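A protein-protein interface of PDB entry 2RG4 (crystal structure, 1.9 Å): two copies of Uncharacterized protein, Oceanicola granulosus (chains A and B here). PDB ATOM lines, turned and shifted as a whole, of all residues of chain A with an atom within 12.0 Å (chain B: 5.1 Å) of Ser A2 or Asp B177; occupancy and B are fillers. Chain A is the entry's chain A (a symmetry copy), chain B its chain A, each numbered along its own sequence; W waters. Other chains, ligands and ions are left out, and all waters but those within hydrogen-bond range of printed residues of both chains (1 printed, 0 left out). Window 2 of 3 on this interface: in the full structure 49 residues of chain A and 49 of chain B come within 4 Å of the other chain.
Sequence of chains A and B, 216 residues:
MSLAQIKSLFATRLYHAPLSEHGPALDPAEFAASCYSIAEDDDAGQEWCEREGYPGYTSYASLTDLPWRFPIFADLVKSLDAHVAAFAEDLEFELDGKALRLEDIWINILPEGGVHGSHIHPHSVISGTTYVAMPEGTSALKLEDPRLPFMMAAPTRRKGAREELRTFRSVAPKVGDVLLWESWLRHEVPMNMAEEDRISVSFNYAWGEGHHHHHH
His B16 touches Leu A3 (O to O, 3.7 Å).
Leu A3 touches Pro B18.
Ala A4 touches His B16 (CA to O, 3.5 Å).
Ala B17 touches Ala A4 (CB to CB, 3.9 Å).
Pro B18 touches Ala A4 (CD to N, 3.8 Å).
A ring nitrogen (NE2) of His B16 sits at hydrogen-bond distance from the side-chain carboxylate of Asp B177.
The backbone carbonyl oxygen (O) of Ala B17 lies within hydrogen-bond range of the backbone NH (N) of Val B178, at 2.7 Å.
N of Tyr B131 sits at hydrogen-bond distance from O of Asp B177 (3.1 Å).
The backbone NH of Lys B174 sits at hydrogen-bond distance from the side-chain carboxylate of Asp B177 (3.2 Å).
The side-chain amide nitrogen (NE2) of Gln A5 lies close to the side-chain amino group (NZ) of Lys A7 (3.2 Å).
O of His B16 lies within hydrogen-bond range of N of Gln A5.
The side-chain carboxylate (OD1) of Asp B177 is in hydrogen-bond range of the side-chain hydroxyl (OG) of Ser A2, at 2.7 Å.
OG of Ser A2 sits close to N of Pro B18.
Of the 6 printed residues of chain A, 4 touch a printed residue of chain B.
Of the 14 printed residues of chain B, 4 touch a printed residue of chain A.
Hydrophobic or aromatic side chains of chain B within 4 Å of the printed part of chain A: Ala B17 and Pro B18.
Among the printed residues, 8 pairs touch across the chains.
Of chain B, only Pro B18 and Asp B177 come within 4 Å of Ser A2.
Of chain A, only Ser A2 (2.7 Å) comes within 4 Å of Asp B177.
Of chain A, only Ser A2, Leu A3 and Ala A4 come within 4 Å of Pro B18.
Leu B19 touches none of the printed residues of chain A.
No residue of chain A comes within 4 Å of Thr B130.
No residue of chain A comes within 4 Å of Tyr B131.
No residue of chain A comes within 4 Å of Pro B173.
No residue of chain A comes within 4 Å of Lys B174.
No residue of chain A comes within 4 Å of Val B175.
No residue of chain A comes within 4 Å of Val B178.
No residue of chain A comes within 4 Å of Leu B179.
Printed residues of chain A within 4 Å of His B16: Leu A3 (3.7 Å), Ala A4 (3.5 Å) and Gln A5 (2.8 Å).
Of the printed residues of chain B, Gln A5 touches His B16 (2.8 Å).
Of the printed residues of chain B, Leu A3 touches His B16 (3.7 Å) and Pro B18 (3.8 Å).
Printed residues of chain B within 4 Å of Ala A4: His B16 (3.5 Å), Ala B17 (3.9 Å) and Pro B18 (3.8 Å).
Ile A6 touches none of the printed residues of chain B.
Lys A7 touches none of the printed residues of chain B.
The nearest residue of chain A that does not touch Asp B177 is Leu A3 (6.3 Å).
Water W1 lies within hydrogen-bond range of O of Leu A3 (2.7 Å) and NE2 of His B16 (3.5 Å).
No position is printed for both chains.
Of the 8 pairs that touch across the chains among the printed residues, none has its exchanged pair printed and touching as well.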
ATOM      1  N   SER A   2     -24.867  22.509  -8.479  1.00  0.00           N
ATOM      2  CA  SER A   2     -25.295  21.114  -8.442  1.00  0.00           C
ATOM      3  C   SER A   2     -26.445  20.917  -7.437  1.00  0.00           C
ATOM      4  O   SER A   2     -26.662  21.776  -6.558  1.00  0.00           O
ATOM      5  CB  SER A   2     -24.087  20.231  -8.156  1.00  0.00           C
ATOM      6  OG  SER A   2     -23.566  20.411  -6.860  1.00  0.00           O
ATOM      7  N   LEU A   3     -27.174  19.821  -7.642  1.00  0.00           N
ATOM      8  CA  LEU A   3     -28.263  19.304  -6.766  1.00  0.00           C
ATOM      9  C   LEU A   3     -27.784  18.112  -6.016  1.00  0.00           C
ATOM     10  O   LEU A   3     -27.063  17.269  -6.606  1.00  0.00           O
ATOM     11  CB  LEU A   3     -29.435  18.763  -7.620  1.00  0.00           C
ATOM     12  CG  LEU A   3     -30.081  19.834  -8.465  1.00  0.00           C
ATOM     13  CD1 LEU A   3     -31.206  19.280  -9.322  1.00  0.00           C
ATOM     14  CD2 LEU A   3     -30.544  20.995  -7.580  1.00  0.00           C
ATOM     15  N   ALA A   4     -28.232  17.978  -4.744  1.00  0.00           N
ATOM     16  CA  ALA A   4     -27.828  16.838  -3.952  1.00  0.00           C
ATOM     17  C   ALA A   4     -28.523  15.632  -4.457  1.00  0.00           C
ATOM     18  O   ALA A   4     -29.733  15.634  -4.657  1.00  0.00           O
ATOM     19  CB  ALA A   4     -28.110  17.018  -2.436  1.00  0.00           C
ATOM     20  N   GLN A   5     -27.729  14.576  -4.643  1.00  0.00           N
ATOM     21  CA  GLN A   5     -28.235  13.339  -5.210  1.00  0.00           C
ATOM     22  C   GLN A   5     -27.600  12.191  -4.391  1.00  0.00           C
ATOM     23  O   GLN A   5     -26.452  12.299  -3.857  1.00  0.00           O
ATOM     24  CB  GLN A   5     -27.963  13.271  -6.753  1.00  0.00           C
ATOM     25  CG  GLN A   5     -28.895  12.307  -7.624  1.00  0.00           C
ATOM     26  CD  GLN A   5     -29.304  12.822  -9.065  1.00  0.00           C
ATOM     27  OE1 GLN A   5     -28.875  13.912  -9.485  1.00  0.00           O
ATOM     28  NE2 GLN A   5     -30.194  12.052  -9.783  1.00  0.00           N
ATOM     29  N   ILE A   6     -28.361  11.106  -4.236  1.00  0.00           N
ATOM     30  CA  ILE A   6     -27.770   9.848  -3.698  1.00  0.00           C
ATOM     31  C   ILE A   6     -28.262   8.743  -4.631  1.00  0.00           C
ATOM     32  O   ILE A   6     -29.458   8.580  -4.771  1.00  0.00           O
ATOM     33  CB  ILE A   6     -28.191   9.465  -2.213  1.00  0.00           C
ATOM     34  CG1 ILE A   6     -28.221  10.690  -1.289  1.00  0.00           C
ATOM     35  CG2 ILE A   6     -27.329   8.347  -1.681  1.00  0.00           C
ATOM     36  CD1 ILE A   6     -28.333  10.378   0.217  1.00  0.00           C
ATOM     37  N   LYS A   7     -27.338   7.973  -5.213  1.00  0.00           N
ATOM     38  CA  LYS A   7     -27.604   6.998  -6.270  1.00  0.00           C
ATOM     39  C   LYS A   7     -27.332   5.568  -5.809  1.00  0.00           C
ATOM     40  O   LYS A   7     -26.407   5.315  -5.033  1.00  0.00           O
ATOM     41  CB  LYS A   7     -26.756   7.277  -7.516  1.00  0.00           C
ATOM     42  CG  LYS A   7     -26.625   8.636  -7.979  1.00  0.00           C
ATOM     43  CD  LYS A   7     -27.921   9.136  -8.517  1.00  0.00           C
ATOM     44  CE  LYS A   7     -28.397   8.340  -9.695  1.00  0.00           C
ATOM     45  NZ  LYS A   7     -29.772   8.867  -9.937  1.00  0.00           N
ATOM     46  N   HIS B  16     -23.634  12.594  -3.664  1.00  0.00           N
ATOM     47  CA  HIS B  16     -23.008  13.568  -4.506  1.00  0.00           C
ATOM     48  C   HIS B  16     -23.824  14.851  -4.282  1.00  0.00           C
ATOM     49  O   HIS B  16     -24.965  14.875  -4.630  1.00  0.00           O
ATOM     50  CB  HIS B  16     -23.023  13.135  -6.003  1.00  0.00           C
ATOM     51  CG  HIS B  16     -22.363  14.100  -6.948  1.00  0.00           C
ATOM     52  ND1 HIS B  16     -22.265  13.844  -8.302  1.00  0.00           N
ATOM     53  CD2 HIS B  16     -21.851  15.344  -6.771  1.00  0.00           C
ATOM     54  CE1 HIS B  16     -21.667  14.857  -8.903  1.00  0.00           C
ATOM     55  NE2 HIS B  16     -21.374  15.765  -7.991  1.00  0.00           N
ATOM     56  N   ALA B  17     -23.216  15.858  -3.646  1.00  0.00           N
ATOM     57  CA  ALA B  17     -23.925  17.059  -3.297  1.00  0.00           C
ATOM     58  C   ALA B  17     -23.029  18.249  -3.489  1.00  0.00           C
ATOM     59  O   ALA B  17     -21.827  18.120  -3.309  1.00  0.00           O
ATOM     60  CB  ALA B  17     -24.294  17.024  -1.857  1.00  0.00           C
ATOM     61  N   PRO B  18     -23.609  19.437  -3.693  1.00  0.00           N
ATOM     62  CA  PRO B  18     -22.747  20.619  -3.432  1.00  0.00           C
ATOM     63  C   PRO B  18     -22.335  20.700  -1.909  1.00  0.00           C
ATOM     64  O   PRO B  18     -23.139  20.409  -0.983  1.00  0.00           O
ATOM     65  CB  PRO B  18     -23.645  21.775  -3.824  1.00  0.00           C
ATOM     66  CG  PRO B  18     -25.103  21.198  -3.552  1.00  0.00           C
ATOM     67  CD  PRO B  18     -25.016  19.808  -4.045  1.00  0.00           C
ATOM     68  N   LEU B  19     -21.083  21.052  -1.651  1.00  0.00           N
ATOM     69  CA  LEU B  19     -20.586  21.209  -0.319  1.00  0.00           C
ATOM     70  C   LEU B  19     -21.486  22.170   0.407  1.00  0.00           C
ATOM     71  O   LEU B  19     -21.720  22.003   1.608  1.00  0.00           O
ATOM     72  CB  LEU B  19     -19.134  21.785  -0.334  1.00  0.00           C
ATOM     73  CG  LEU B  19     -18.438  22.012   1.031  1.00  0.00           C
ATOM     74  CD1 LEU B  19     -18.276  20.633   1.717  1.00  0.00           C
ATOM     75  CD2 LEU B  19     -17.083  22.819   0.845  1.00  0.00           C
ATOM     76  N   THR B 129     -14.501  12.978  -0.920  1.00  0.00           N
ATOM     77  CA  THR B 129     -13.598  13.957  -1.474  1.00  0.00           C
ATOM     78  C   THR B 129     -14.448  15.189  -1.765  1.00  0.00           C
ATOM     79  O   THR B 129     -15.573  14.981  -2.147  1.00  0.00           O
ATOM     80  CB  THR B 129     -13.075  13.432  -2.877  1.00  0.00           C
ATOM     81  OG1 THR B 129     -12.191  12.343  -2.657  1.00  0.00           O
ATOM     82  CG2 THR B 129     -12.216  14.517  -3.509  1.00  0.00           C
ATOM     83  N   THR B 130     -13.973  16.429  -1.473  1.00  0.00           N
ATOM     84  CA  THR B 130     -14.567  17.625  -2.076  1.00  0.00           C
ATOM     85  C   THR B 130     -13.562  18.236  -3.044  1.00  0.00           C
ATOM     86  O   THR B 130     -12.388  18.086  -2.854  1.00  0.00           O
ATOM     87  CB  THR B 130     -14.715  18.842  -1.164  1.00  0.00           C
ATOM     88  OG1 THR B 130     -14.259  18.680   0.178  1.00  0.00           O
ATOM     89  CG2 THR B 130     -15.912  19.520  -1.335  1.00  0.00           C
ATOM     90  N   TYR B 131     -14.036  19.034  -4.017  1.00  0.00           N
ATOM     91  CA  TYR B 131     -13.230  19.407  -5.197  1.00  0.00           C
ATOM     92  C   TYR B 131     -13.007  20.858  -5.027  1.00  0.00           C
ATOM     93  O   TYR B 131     -13.963  21.600  -4.809  1.00  0.00           O
ATOM     94  CB  TYR B 131     -13.959  19.064  -6.516  1.00  0.00           C
ATOM     95  CG  TYR B 131     -14.008  17.534  -6.589  1.00  0.00           C
ATOM     96  CD1 TYR B 131     -12.916  16.842  -7.138  1.00  0.00           C
ATOM     97  CD2 TYR B 131     -14.988  16.807  -5.950  1.00  0.00           C
ATOM     98  CE1 TYR B 131     -12.848  15.475  -7.108  1.00  0.00           C
ATOM     99  CE2 TYR B 131     -14.933  15.355  -5.933  1.00  0.00           C
ATOM    100  CZ  TYR B 131     -13.845  14.745  -6.531  1.00  0.00           C
ATOM    101  OH  TYR B 131     -13.681  13.394  -6.583  1.00  0.00           O
ATOM    102  N   PRO B 173     -17.451  15.487 -11.208  1.00  0.00           N
ATOM    103  CA  PRO B 173     -17.847  16.548 -10.271  1.00  0.00           C
ATOM    104  C   PRO B 173     -17.469  17.910 -10.821  1.00  0.00           C
ATOM    105  O   PRO B 173     -16.627  17.990 -11.741  1.00  0.00           O
ATOM    106  CB  PRO B 173     -16.951  16.277  -9.056  1.00  0.00           C
ATOM    107  CG  PRO B 173     -16.409  14.868  -9.245  1.00  0.00           C
ATOM    108  CD  PRO B 173     -16.261  14.759 -10.721  1.00  0.00           C
ATOM    109  N   LYS B 174     -18.011  18.978 -10.206  1.00  0.00           N
ATOM    110  CA  LYS B 174     -17.617  20.354 -10.534  1.00  0.00           C
ATOM    111  C   LYS B 174     -16.906  20.836  -9.270  1.00  0.00           C
ATOM    112  O   LYS B 174     -17.126  20.225  -8.201  1.00  0.00           O
ATOM    113  CB  LYS B 174     -18.876  21.185 -10.714  1.00  0.00           C
ATOM    114  CG  LYS B 174     -20.028  20.485 -11.364  1.00  0.00           C
ATOM    115  CD  LYS B 174     -20.337  21.078 -12.727  1.00  0.00           C
ATOM    116  CE  LYS B 174     -19.765  20.237 -13.888  1.00  0.00           C
ATOM    117  NZ  LYS B 174     -20.339  20.650 -15.233  1.00  0.00           N
ATOM    118  N   VAL B 175     -16.107  21.921  -9.340  1.00  0.00           N
ATOM    119  CA  VAL B 175     -15.703  22.602  -8.120  1.00  0.00           C
ATOM    120  C   VAL B 175     -16.883  22.842  -7.217  1.00  0.00           C
ATOM    121  O   VAL B 175     -18.027  23.200  -7.695  1.00  0.00           O
ATOM    122  CB  VAL B 175     -14.978  23.962  -8.336  1.00  0.00           C
ATOM    123  CG1 VAL B 175     -13.530  23.710  -8.497  1.00  0.00           C
ATOM    124  CG2 VAL B 175     -15.594  24.688  -9.506  1.00  0.00           C
ATOM    125  N   GLY B 176     -16.607  22.733  -5.920  1.00  0.00           N
ATOM    126  CA  GLY B 176     -17.614  22.850  -4.897  1.00  0.00           C
ATOM    127  C   GLY B 176     -18.382  21.598  -4.539  1.00  0.00           C
ATOM    128  O   GLY B 176     -19.122  21.623  -3.568  1.00  0.00           O
ATOM    129  N   ASP B 177     -18.239  20.491  -5.294  1.00  0.00           N
ATOM    130  CA  ASP B 177     -19.064  19.321  -5.032  1.00  0.00           C
ATOM    131  C   ASP B 177     -18.331  18.525  -3.995  1.00  0.00           C
ATOM    132  O   ASP B 177     -17.080  18.587  -3.920  1.00  0.00           O
ATOM    133  CB  ASP B 177     -19.193  18.421  -6.282  1.00  0.00           C
ATOM    134  CG  ASP B 177     -20.273  18.880  -7.232  1.00  0.00           C
ATOM    135  OD1 ASP B 177     -20.928  19.912  -6.946  1.00  0.00           O
ATOM    136  OD2 ASP B 177     -20.452  18.181  -8.286  1.00  0.00           O
ATOM    137  N   VAL B 178     -19.110  17.777  -3.222  1.00  0.00           N
ATOM    138  CA  VAL B 178     -18.581  16.767  -2.319  1.00  0.00           C
ATOM    139  C   VAL B 178     -19.152  15.388  -2.753  1.00  0.00           C
ATOM    140  O   VAL B 178     -20.361  15.247  -3.048  1.00  0.00           O
ATOM    141  CB  VAL B 178     -18.892  17.067  -0.785  1.00  0.00           C
ATOM    142  CG1 VAL B 178     -20.287  17.214  -0.538  1.00  0.00           C
ATOM    143  CG2 VAL B 178     -18.393  15.940   0.131  1.00  0.00           C
ATOM    144  N   LEU B 179     -18.271  14.397  -2.852  1.00  0.00           N
ATOM    145  CA  LEU B 179     -18.656  12.976  -2.961  1.00  0.00           C
ATOM    146  C   LEU B 179     -18.382  12.159  -1.664  1.00  0.00           C
ATOM    147  O   LEU B 179     -17.342  12.314  -1.035  1.00  0.00           O
ATOM    148  CB  LEU B 179     -17.884  12.337  -4.118  1.00  0.00           C
ATOM    149  CG  LEU B 179     -18.161  12.990  -5.504  1.00  0.00           C
ATOM    150  CD1 LEU B 179     -17.113  12.548  -6.532  1.00  0.00           C
ATOM    151  CD2 LEU B 179     -19.451  12.538  -5.927  1.00  0.00           C
HETATM  152  O   HOH W   1     -24.506  17.036  -7.295  1.00  0.00           O
